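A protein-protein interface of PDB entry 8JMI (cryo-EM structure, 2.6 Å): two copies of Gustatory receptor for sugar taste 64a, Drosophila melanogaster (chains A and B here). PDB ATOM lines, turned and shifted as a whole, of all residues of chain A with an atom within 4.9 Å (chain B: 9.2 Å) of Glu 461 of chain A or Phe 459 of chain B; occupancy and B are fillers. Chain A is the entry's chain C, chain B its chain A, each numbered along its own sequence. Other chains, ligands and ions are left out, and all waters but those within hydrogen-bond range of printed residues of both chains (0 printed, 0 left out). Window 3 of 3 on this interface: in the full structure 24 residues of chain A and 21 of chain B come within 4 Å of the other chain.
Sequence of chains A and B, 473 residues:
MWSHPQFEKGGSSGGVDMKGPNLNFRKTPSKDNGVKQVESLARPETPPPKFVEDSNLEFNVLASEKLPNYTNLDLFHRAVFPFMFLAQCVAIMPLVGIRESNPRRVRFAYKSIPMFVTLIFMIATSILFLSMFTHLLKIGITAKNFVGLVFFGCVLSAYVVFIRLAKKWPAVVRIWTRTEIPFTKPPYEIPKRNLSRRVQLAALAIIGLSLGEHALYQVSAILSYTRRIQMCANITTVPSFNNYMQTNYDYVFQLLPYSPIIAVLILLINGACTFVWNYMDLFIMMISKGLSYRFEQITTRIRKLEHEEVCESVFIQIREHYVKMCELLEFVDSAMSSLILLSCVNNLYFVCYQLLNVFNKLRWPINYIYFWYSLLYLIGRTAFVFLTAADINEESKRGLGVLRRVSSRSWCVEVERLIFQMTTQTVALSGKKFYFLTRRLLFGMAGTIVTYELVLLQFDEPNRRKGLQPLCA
NE2 of Gln 458 of chain A is in hydrogen-bond range of O of Val 455 of chain B (3.1 Å).
NE2 of Gln 458 of chain A sits at hydrogen-bond distance from OE1 of Gln 458 of chain B (3.1 Å).
OE1 of Gln 458 of chain B sits close to O of Val 455 of chain B (3.1 Å).
O of Leu 454 of chain A lies within hydrogen-bond range of NE2 of Gln 458 of chain A, 3.4 Å away.
Of the printed residues of chain B, Leu 457 of chain A touches Phe 459 (3.5 Å).
No residue of chain B comes within 4 Å of Asp 460 of chain A.
Glu 461 of chain A touches just one residue of chain B: Phe 459 (3.4 Å).
No residue of chain B comes within 4 Å of Arg 464 of chain A.
Printed residues of chain A within 4 Å of Val 455 of chain B: Leu 454 (3.6 Å) and Gln 458 (3.1 Å).
Of the printed residues of chain A, Leu 456 of chain B touches Leu 454 (3.6 Å).
Phe 459 of chain B touches just these residues of chain A: Leu 454, Leu 457, Gln 458 and Glu 461.
Arg 464 of chain B touches none of the printed residues of chain A.
The nearest printed residue of chain A that does not touch Val 455 of chain B is Leu 457 of chain A (7.4 Å).
Hydrophobic or aromatic side chains of chain B within 4 Å of the printed part of chain A: Tyr 452, Val 455, Leu 456 and Phe 459.
Of the 10 printed residues of chain A, 4 touch a printed residue of chain B.
Among the printed residues, no Asp or Glu carboxylate lies within 4 Å of a Lys or Arg side-chain nitrogen of the other chain.
Among the printed residues, pairs that only touch across the chains: Leu 454 of chain A with Tyr 452 of chain B, Leu 454 of chain A with Val 455 of chain B, Leu 454 of chain A with Leu 456 of chain B, Leu 454 of chain A with Phe 459 of chain B, Leu 457 of chain A with Phe 459 of chain B, Gln 458 of chain A with Phe 459 of chain B and Glu 461 of chain A with Phe 459 of chain B.
Leu 457 of chain A touches Phe 459 of chain B, but with the chains exchanged Phe 459 of chain A does not touch Leu 457 of chain B (12.9 Å).
Gln 458 of chain B touches its own counterpart, Gln 458 of chain A.
Gln 458 of chain A touches Phe 459 of chain B, but with the chains exchanged Phe 459 of chain A does not touch Gln 458 of chain B (8.8 Å).
Glu 461 of chain A touches Phe 459 of chain B, but with the chains exchanged Phe 459 of chain A does not touch Glu 461 of chain B (12.4 Å).
10 positions are printed for both chains.
Of the 9 pairs that touch across the chains among the printed residues, 1 has its exchanged pair printed and touching as well.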
ATOM      1  N   LEU A 454     -18.509 -34.397  11.772  1.00  0.00           N
ATOM      2  CA  LEU A 454     -19.030 -33.169  11.183  1.00  0.00           C
ATOM      3  C   LEU A 454     -20.382 -32.808  11.783  1.00  0.00           C
ATOM      4  O   LEU A 454     -20.639 -31.640  12.094  1.00  0.00           O
ATOM      5  CB  LEU A 454     -19.143 -33.318   9.666  1.00  0.00           C
ATOM      6  CG  LEU A 454     -17.844 -33.286   8.856  1.00  0.00           C
ATOM      7  CD1 LEU A 454     -18.148 -33.393   7.371  1.00  0.00           C
ATOM      8  CD2 LEU A 454     -17.044 -32.028   9.147  1.00  0.00           C
ATOM      9  N   LEU A 457     -19.795 -31.924  15.828  1.00  0.00           N
ATOM     10  CA  LEU A 457     -19.039 -30.753  16.252  1.00  0.00           C
ATOM     11  C   LEU A 457     -19.942 -29.549  16.472  1.00  0.00           C
ATOM     12  O   LEU A 457     -19.535 -28.595  17.143  1.00  0.00           O
ATOM     13  CB  LEU A 457     -17.956 -30.427  15.223  1.00  0.00           C
ATOM     14  CG  LEU A 457     -16.675 -31.259  15.323  1.00  0.00           C
ATOM     15  CD1 LEU A 457     -15.827 -31.077  14.077  1.00  0.00           C
ATOM     16  CD2 LEU A 457     -15.883 -30.894  16.570  1.00  0.00           C
ATOM     17  N   GLN A 458     -21.155 -29.573  15.920  1.00  0.00           N
ATOM     18  CA  GLN A 458     -22.137 -28.538  16.216  1.00  0.00           C
ATOM     19  C   GLN A 458     -22.725 -28.703  17.611  1.00  0.00           C
ATOM     20  O   GLN A 458     -23.064 -27.706  18.260  1.00  0.00           O
ATOM     21  CB  GLN A 458     -23.251 -28.566  15.170  1.00  0.00           C
ATOM     22  CG  GLN A 458     -22.764 -28.251  13.752  1.00  0.00           C
ATOM     23  CD  GLN A 458     -23.361 -29.135  12.650  1.00  0.00           C
ATOM     24  OE1 GLN A 458     -24.323 -29.861  12.900  1.00  0.00           O
ATOM     25  NE2 GLN A 458     -22.778 -29.110  11.452  1.00  0.00           N
ATOM     26  N   PHE A 459     -22.856 -29.944  18.086  1.00  0.00           N
ATOM     27  CA  PHE A 459     -23.416 -30.179  19.413  1.00  0.00           C
ATOM     28  C   PHE A 459     -22.554 -29.540  20.495  1.00  0.00           C
ATOM     29  O   PHE A 459     -23.069 -28.898  21.418  1.00  0.00           O
ATOM     30  CB  PHE A 459     -23.549 -31.681  19.662  1.00  0.00           C
ATOM     31  CG  PHE A 459     -24.782 -32.291  19.064  1.00  0.00           C
ATOM     32  CD1 PHE A 459     -24.789 -32.708  17.746  1.00  0.00           C
ATOM     33  CD2 PHE A 459     -25.926 -32.462  19.824  1.00  0.00           C
ATOM     34  CE1 PHE A 459     -25.918 -33.274  17.191  1.00  0.00           C
ATOM     35  CE2 PHE A 459     -27.058 -33.030  19.274  1.00  0.00           C
ATOM     36  CZ  PHE A 459     -27.053 -33.437  17.955  1.00  0.00           C
ATOM     37  N   ASP A 460     -21.237 -29.703  20.395  1.00  0.00           N
ATOM     38  CA  ASP A 460     -20.316 -29.257  21.431  1.00  0.00           C
ATOM     39  C   ASP A 460     -19.708 -27.891  21.145  1.00  0.00           C
ATOM     40  O   ASP A 460     -18.804 -27.470  21.875  1.00  0.00           O
ATOM     41  CB  ASP A 460     -19.193 -30.285  21.613  1.00  0.00           C
ATOM     42  CG  ASP A 460     -18.106 -30.152  20.563  1.00  0.00           C
ATOM     43  OD1 ASP A 460     -18.442 -29.894  19.388  1.00  0.00           O
ATOM     44  OD2 ASP A 460     -16.918 -30.305  20.914  1.00  0.00           O
ATOM     45  N   GLU A 461     -20.170 -27.192  20.109  1.00  0.00           N
ATOM     46  CA  GLU A 461     -19.672 -25.844  19.843  1.00  0.00           C
ATOM     47  C   GLU A 461     -19.829 -24.921  21.042  1.00  0.00           C
ATOM     48  O   GLU A 461     -18.862 -24.219  21.384  1.00  0.00           O
ATOM     49  CB  GLU A 461     -20.389 -25.268  18.615  1.00  0.00           C
ATOM     50  CG  GLU A 461     -19.541 -25.265  17.351  1.00  0.00           C
ATOM     51  CD  GLU A 461     -20.366 -25.095  16.090  1.00  0.00           C
ATOM     52  OE1 GLU A 461     -21.608 -25.199  16.167  1.00  0.00           O
ATOM     53  OE2 GLU A 461     -19.770 -24.856  15.017  1.00  0.00           O
ATOM     54  N   PRO A 462     -20.986 -24.859  21.711  1.00  0.00           N
ATOM     55  CA  PRO A 462     -21.058 -24.063  22.947  1.00  0.00           C
ATOM     56  C   PRO A 462     -20.019 -24.480  23.971  1.00  0.00           C
ATOM     57  O   PRO A 462     -19.362 -23.622  24.574  1.00  0.00           O
ATOM     58  CB  PRO A 462     -22.489 -24.316  23.442  1.00  0.00           C
ATOM     59  CG  PRO A 462     -23.254 -24.711  22.226  1.00  0.00           C
ATOM     60  CD  PRO A 462     -22.287 -25.448  21.349  1.00  0.00           C
ATOM     61  N   ASN A 463     -19.828 -25.789  24.157  1.00  0.00           N
ATOM     62  CA  ASN A 463     -18.825 -26.264  25.103  1.00  0.00           C
ATOM     63  C   ASN A 463     -17.427 -25.842  24.673  1.00  0.00           C
ATOM     64  O   ASN A 463     -16.602 -25.458  25.512  1.00  0.00           O
ATOM     65  CB  ASN A 463     -18.909 -27.784  25.235  1.00  0.00           C
ATOM     66  CG  ASN A 463     -20.287 -28.257  25.653  1.00  0.00           C
ATOM     67  OD1 ASN A 463     -21.114 -28.613  24.812  1.00  0.00           O
ATOM     68  ND2 ASN A 463     -20.542 -28.263  26.955  1.00  0.00           N
ATOM     69  N   ARG A 464     -17.139 -25.913  23.373  1.00  0.00           N
ATOM     70  CA  ARG A 464     -15.828 -25.500  22.887  1.00  0.00           C
ATOM     71  C   ARG A 464     -15.589 -24.019  23.147  1.00  0.00           C
ATOM     72  O   ARG A 464     -14.482 -23.619  23.528  1.00  0.00           O
ATOM     73  CB  ARG A 464     -15.698 -25.818  21.398  1.00  0.00           C
ATOM     74  CG  ARG A 464     -15.318 -27.264  21.116  1.00  0.00           C
ATOM     75  CD  ARG A 464     -15.569 -27.644  19.667  1.00  0.00           C
ATOM     76  NE  ARG A 464     -14.841 -26.782  18.742  1.00  0.00           N
ATOM     77  CZ  ARG A 464     -15.238 -26.491  17.510  1.00  0.00           C
ATOM     78  NH1 ARG A 464     -16.360 -26.984  17.008  1.00  0.00           N
ATOM     79  NH2 ARG A 464     -14.489 -25.687  16.760  1.00  0.00           N
ATOM     80  N   ARG A 465     -16.613 -23.185  22.948  1.00  0.00           N
ATOM     81  CA  ARG A 465     -16.450 -21.758  23.209  1.00  0.00           C
ATOM     82  C   ARG A 465     -16.507 -21.417  24.694  1.00  0.00           C
ATOM     83  O   ARG A 465     -16.176 -20.284  25.058  1.00  0.00           O
ATOM     84  CB  ARG A 465     -17.508 -20.950  22.453  1.00  0.00           C
ATOM     85  CG  ARG A 465     -18.937 -21.276  22.828  1.00  0.00           C
ATOM     86  CD  ARG A 465     -19.920 -20.328  22.154  1.00  0.00           C
ATOM     87  NE  ARG A 465     -21.229 -20.344  22.802  1.00  0.00           N
ATOM     88  CZ  ARG A 465     -22.343 -20.825  22.263  1.00  0.00           C
ATOM     89  NH1 ARG A 465     -22.359 -21.351  21.048  1.00  0.00           N
ATOM     90  NH2 ARG A 465     -23.472 -20.779  22.964  1.00  0.00           N
ATOM     91  N   ALA B 143      -9.688 -22.335  10.761  1.00  0.00           N
ATOM     92  CA  ALA B 143     -10.000 -23.260   9.677  1.00  0.00           C
ATOM     93  C   ALA B 143      -9.662 -22.659   8.321  1.00  0.00           C
ATOM     94  O   ALA B 143      -9.280 -23.386   7.397  1.00  0.00           O
ATOM     95  CB  ALA B 143     -11.477 -23.652   9.728  1.00  0.00           C
ATOM     96  N   LYS B 144      -9.792 -21.339   8.180  1.00  0.00           N
ATOM     97  CA  LYS B 144      -9.435 -20.685   6.928  1.00  0.00           C
ATOM     98  C   LYS B 144      -7.926 -20.571   6.756  1.00  0.00           C
ATOM     99  O   LYS B 144      -7.419 -20.760   5.645  1.00  0.00           O
ATOM    100  CB  LYS B 144     -10.079 -19.298   6.862  1.00  0.00           C
ATOM    101  CG  LYS B 144     -11.606 -19.304   6.821  1.00  0.00           C
ATOM    102  CD  LYS B 144     -12.167 -20.253   5.766  1.00  0.00           C
ATOM    103  CE  LYS B 144     -13.687 -20.214   5.733  1.00  0.00           C
ATOM    104  NZ  LYS B 144     -14.285 -21.167   6.709  1.00  0.00           N
ATOM    105  N   LEU B 356     -16.767 -24.562   0.305  1.00  0.00           N
ATOM    106  CA  LEU B 356     -17.299 -23.875   1.473  1.00  0.00           C
ATOM    107  C   LEU B 356     -17.203 -22.360   1.347  1.00  0.00           C
ATOM    108  O   LEU B 356     -17.842 -21.645   2.125  1.00  0.00           O
ATOM    109  CB  LEU B 356     -16.560 -24.341   2.731  1.00  0.00           C
ATOM    110  CG  LEU B 356     -17.381 -24.522   4.011  1.00  0.00           C
ATOM    111  CD1 LEU B 356     -18.559 -25.462   3.805  1.00  0.00           C
ATOM    112  CD2 LEU B 356     -16.487 -25.027   5.132  1.00  0.00           C
ATOM    113  N   THR B 451     -22.703 -34.043   0.762  1.00  0.00           N
ATOM    114  CA  THR B 451     -23.118 -34.202   2.155  1.00  0.00           C
ATOM    115  C   THR B 451     -22.234 -33.382   3.088  1.00  0.00           C
ATOM    116  O   THR B 451     -22.728 -32.693   3.993  1.00  0.00           O
ATOM    117  CB  THR B 451     -23.085 -35.682   2.542  1.00  0.00           C
ATOM    118  OG1 THR B 451     -24.136 -36.380   1.864  1.00  0.00           O
ATOM    119  CG2 THR B 451     -23.253 -35.852   4.046  1.00  0.00           C
ATOM    120  N   TYR B 452     -20.916 -33.444   2.882  1.00  0.00           N
ATOM    121  CA  TYR B 452     -20.001 -32.680   3.720  1.00  0.00           C
ATOM    122  C   TYR B 452     -20.252 -31.186   3.586  1.00  0.00           C
ATOM    123  O   TYR B 452     -20.234 -30.460   4.583  1.00  0.00           O
ATOM    124  CB  TYR B 452     -18.549 -33.008   3.360  1.00  0.00           C
ATOM    125  CG  TYR B 452     -18.094 -34.404   3.732  1.00  0.00           C
ATOM    126  CD1 TYR B 452     -18.931 -35.282   4.411  1.00  0.00           C
ATOM    127  CD2 TYR B 452     -16.817 -34.842   3.407  1.00  0.00           C
ATOM    128  CE1 TYR B 452     -18.510 -36.552   4.750  1.00  0.00           C
ATOM    129  CE2 TYR B 452     -16.388 -36.112   3.742  1.00  0.00           C
ATOM    130  CZ  TYR B 452     -17.238 -36.961   4.415  1.00  0.00           C
ATOM    131  OH  TYR B 452     -16.816 -38.227   4.750  1.00  0.00           O
ATOM    132  N   GLU B 453     -20.483 -30.706   2.364  1.00  0.00           N
ATOM    133  CA  GLU B 453     -20.752 -29.286   2.165  1.00  0.00           C
ATOM    134  C   GLU B 453     -22.055 -28.876   2.836  1.00  0.00           C
ATOM    135  O   GLU B 453     -22.132 -27.804   3.447  1.00  0.00           O
ATOM    136  CB  GLU B 453     -20.795 -28.961   0.672  1.00  0.00           C
ATOM    137  CG  GLU B 453     -19.437 -28.970  -0.015  1.00  0.00           C
ATOM    138  CD  GLU B 453     -18.420 -28.088   0.682  1.00  0.00           C
ATOM    139  OE1 GLU B 453     -18.668 -26.870   0.800  1.00  0.00           O
ATOM    140  OE2 GLU B 453     -17.376 -28.615   1.117  1.00  0.00           O
ATOM    141  N   LEU B 454     -23.090 -29.710   2.733  1.00  0.00           N
ATOM    142  CA  LEU B 454     -24.353 -29.394   3.390  1.00  0.00           C
ATOM    143  C   LEU B 454     -24.171 -29.298   4.899  1.00  0.00           C
ATOM    144  O   LEU B 454     -24.707 -28.385   5.539  1.00  0.00           O
ATOM    145  CB  LEU B 454     -25.405 -30.450   3.047  1.00  0.00           C
ATOM    146  CG  LEU B 454     -26.003 -30.415   1.638  1.00  0.00           C
ATOM    147  CD1 LEU B 454     -27.064 -31.493   1.492  1.00  0.00           C
ATOM    148  CD2 LEU B 454     -26.586 -29.047   1.321  1.00  0.00           C
ATOM    149  N   VAL B 455     -23.417 -30.228   5.486  1.00  0.00           N
ATOM    150  CA  VAL B 455     -23.224 -30.207   6.933  1.00  0.00           C
ATOM    151  C   VAL B 455     -22.312 -29.054   7.345  1.00  0.00           C
ATOM    152  O   VAL B 455     -22.454 -28.495   8.438  1.00  0.00           O
ATOM    153  CB  VAL B 455     -22.679 -31.562   7.420  1.00  0.00           C
ATOM    154  CG1 VAL B 455     -22.431 -31.523   8.919  1.00  0.00           C
ATOM    155  CG2 VAL B 455     -23.653 -32.678   7.077  1.00  0.00           C
ATOM    156  N   LEU B 456     -21.365 -28.678   6.483  1.00  0.00           N
ATOM    157  CA  LEU B 456     -20.336 -27.719   6.868  1.00  0.00           C
ATOM    158  C   LEU B 456     -20.752 -26.277   6.614  1.00  0.00           C
ATOM    159  O   LEU B 456     -20.218 -25.366   7.255  1.00  0.00           O
ATOM    160  CB  LEU B 456     -19.040 -28.016   6.112  1.00  0.00           C
ATOM    161  CG  LEU B 456     -18.172 -29.144   6.666  1.00  0.00           C
ATOM    162  CD1 LEU B 456     -17.137 -29.567   5.638  1.00  0.00           C
ATOM    163  CD2 LEU B 456     -17.498 -28.712   7.957  1.00  0.00           C
ATOM    164  N   LEU B 457     -21.682 -26.040   5.689  1.00  0.00           N
ATOM    165  CA  LEU B 457     -22.114 -24.674   5.428  1.00  0.00           C
ATOM    166  C   LEU B 457     -22.775 -24.049   6.647  1.00  0.00           C
ATOM    167  O   LEU B 457     -22.884 -22.820   6.718  1.00  0.00           O
ATOM    168  CB  LEU B 457     -23.066 -24.647   4.230  1.00  0.00           C
ATOM    169  CG  LEU B 457     -22.406 -24.670   2.847  1.00  0.00           C
ATOM    170  CD1 LEU B 457     -23.439 -24.961   1.771  1.00  0.00           C
ATOM    171  CD2 LEU B 457     -21.686 -23.362   2.552  1.00  0.00           C
ATOM    172  N   GLN B 458     -23.211 -24.862   7.610  1.00  0.00           N
ATOM    173  CA  GLN B 458     -23.674 -24.319   8.881  1.00  0.00           C
ATOM    174  C   GLN B 458     -22.517 -23.804   9.727  1.00  0.00           C
ATOM    175  O   GLN B 458     -22.678 -22.817  10.454  1.00  0.00           O
ATOM    176  CB  GLN B 458     -24.448 -25.381   9.661  1.00  0.00           C
ATOM    177  CG  GLN B 458     -25.717 -25.857   8.974  1.00  0.00           C
ATOM    178  CD  GLN B 458     -25.904 -27.368   9.063  1.00  0.00           C
ATOM    179  OE1 GLN B 458     -25.209 -28.051   9.816  1.00  0.00           O
ATOM    180  NE2 GLN B 458     -26.852 -27.894   8.291  1.00  0.00           N
ATOM    181  N   PHE B 459     -21.354 -24.455   9.648  1.00  0.00           N
ATOM    182  CA  PHE B 459     -20.212 -24.044  10.458  1.00  0.00           C
ATOM    183  C   PHE B 459     -19.785 -22.618  10.128  1.00  0.00           C
ATOM    184  O   PHE B 459     -19.513 -21.814  11.028  1.00  0.00           O
ATOM    185  CB  PHE B 459     -19.043 -25.005  10.241  1.00  0.00           C
ATOM    186  CG  PHE B 459     -19.126 -26.261  11.055  1.00  0.00           C
ATOM    187  CD1 PHE B 459     -19.847 -27.348  10.596  1.00  0.00           C
ATOM    188  CD2 PHE B 459     -18.471 -26.362  12.271  1.00  0.00           C
ATOM    189  CE1 PHE B 459     -19.923 -28.509  11.337  1.00  0.00           C
ATOM    190  CE2 PHE B 459     -18.544 -27.522  13.017  1.00  0.00           C
ATOM    191  CZ  PHE B 459     -19.271 -28.597  12.547  1.00  0.00           C
ATOM    192  N   ASP B 460     -19.717 -22.288   8.840  1.00  0.00           N
ATOM    193  CA  ASP B 460     -19.202 -21.003   8.390  1.00  0.00           C
ATOM    194  C   ASP B 460     -20.295 -19.977   8.126  1.00  0.00           C
ATOM    195  O   ASP B 460     -19.995 -18.900   7.603  1.00  0.00           O
ATOM    196  CB  ASP B 460     -18.363 -21.191   7.123  1.00  0.00           C
ATOM    197  CG  ASP B 460     -19.212 -21.308   5.874  1.00  0.00           C
ATOM    198  OD1 ASP B 460     -20.280 -21.952   5.939  1.00  0.00           O
ATOM    199  OD2 ASP B 460     -18.813 -20.754   4.827  1.00  0.00           O
ATOM    200  N   GLU B 461     -21.547 -20.279   8.464  1.00  0.00           N
ATOM    201  CA  GLU B 461     -22.617 -19.296   8.301  1.00  0.00           C
ATOM    202  C   GLU B 461     -22.320 -17.989   9.020  1.00  0.00           C
ATOM    203  O   GLU B 461     -22.494 -16.921   8.409  1.00  0.00           O
ATOM    204  CB  GLU B 461     -23.942 -19.896   8.791  1.00  0.00           C
ATOM    205  CG  GLU B 461     -24.877 -20.326   7.668  1.00  0.00           C
ATOM    206  CD  GLU B 461     -25.965 -21.273   8.138  1.00  0.00           C
ATOM    207  OE1 GLU B 461     -25.872 -21.775   9.279  1.00  0.00           O
ATOM    208  OE2 GLU B 461     -26.915 -21.518   7.365  1.00  0.00           O
ATOM    209  N   PRO B 462     -21.885 -17.988  10.284  1.00  0.00           N
ATOM    210  CA  PRO B 462     -21.473 -16.716  10.900  1.00  0.00           C
ATOM    211  C   PRO B 462     -20.399 -16.001  10.101  1.00  0.00           C
ATOM    212  O   PRO B 462     -20.488 -14.785   9.889  1.00  0.00           O
ATOM    213  CB  PRO B 462     -20.971 -17.144  12.286  1.00  0.00           C
ATOM    214  CG  PRO B 462     -21.652 -18.442  12.559  1.00  0.00           C
ATOM    215  CD  PRO B 462     -21.807 -19.115  11.229  1.00  0.00           C
ATOM    216  N   ASN B 463     -19.397 -16.740   9.619  1.00  0.00           N
ATOM    217  CA  ASN B 463     -18.345 -16.127   8.816  1.00  0.00           C
ATOM    218  C   ASN B 463     -18.907 -15.553   7.524  1.00  0.00           C
ATOM    219  O   ASN B 463     -18.503 -14.466   7.091  1.00  0.00           O
ATOM    220  CB  ASN B 463     -17.252 -17.152   8.514  1.00  0.00           C
ATOM    221  CG  ASN B 463     -16.662 -17.762   9.771  1.00  0.00           C
ATOM    222  OD1 ASN B 463     -17.085 -18.830  10.212  1.00  0.00           O
ATOM    223  ND2 ASN B 463     -15.681 -17.084  10.355  1.00  0.00           N
ATOM    224  N   ARG B 464     -19.836 -16.271   6.889  1.00  0.00           N
ATOM    225  CA  ARG B 464     -20.439 -15.769   5.660  1.00  0.00           C
ATOM    226  C   ARG B 464     -21.206 -14.478   5.912  1.00  0.00           C
ATOM    227  O   ARG B 464     -21.150 -13.546   5.100  1.00  0.00           O
ATOM    228  CB  ARG B 464     -21.354 -16.834   5.054  1.00  0.00           C
ATOM    229  CG  ARG B 464     -20.610 -17.876   4.234  1.00  0.00           C
ATOM    230  CD  ARG B 464     -21.463 -19.106   3.973  1.00  0.00           C
ATOM    231  NE  ARG B 464     -22.706 -18.774   3.287  1.00  0.00           N
ATOM    232  CZ  ARG B 464     -23.839 -19.457   3.403  1.00  0.00           C
ATOM    233  NH1 ARG B 464     -23.926 -20.531   4.170  1.00  0.00           N
ATOM    234  NH2 ARG B 464     -24.911 -19.052   2.728  1.00  0.00           N
ATOM    235  N   ARG B 465     -21.929 -14.398   7.033  1.00  0.00           N
ATOM    236  CA  ARG B 465     -22.661 -13.175   7.341  1.00  0.00           C
ATOM    237  C   ARG B 465     -21.763 -12.068   7.885  1.00  0.00           C
ATOM    238  O   ARG B 465     -22.221 -10.925   7.986  1.00  0.00           O
ATOM    239  CB  ARG B 465     -23.789 -13.460   8.335  1.00  0.00           C
ATOM    240  CG  ARG B 465     -23.331 -14.011   9.668  1.00  0.00           C
ATOM    241  CD  ARG B 465     -24.486 -14.120  10.653  1.00  0.00           C
ATOM    242  NE  ARG B 465     -24.020 -14.243  12.032  1.00  0.00           N
ATOM    243  CZ  ARG B 465     -24.142 -15.329  12.786  1.00  0.00           C
ATOM    244  NH1 ARG B 465     -24.716 -16.433  12.332  1.00  0.00           N
ATOM    245  NH2 ARG B 465     -23.672 -15.309  14.030  1.00  0.00           N
ATOM    246  N   LYS B 466     -20.509 -12.368   8.237  1.00  0.00           N
ATOM    247  CA  LYS B 466     -19.583 -11.295   8.593  1.00  0.00           C
ATOM    248  C   LYS B 466     -19.417 -10.315   7.439  1.00  0.00           C
ATOM    249  O   LYS B 466     -19.414  -9.095   7.645  1.00  0.00           O
ATOM    250  CB  LYS B 466     -18.221 -11.867   8.996  1.00  0.00           C
ATOM    251  CG  LYS B 466     -18.199 -12.623  10.315  1.00  0.00           C
ATOM    252  CD  LYS B 466     -18.374 -11.696  11.507  1.00  0.00           C
ATOM    253  CE  LYS B 466     -18.607 -12.479  12.788  1.00  0.00           C
ATOM    254  NZ  LYS B 466     -17.418 -13.288  13.175  1.00  0.00           N
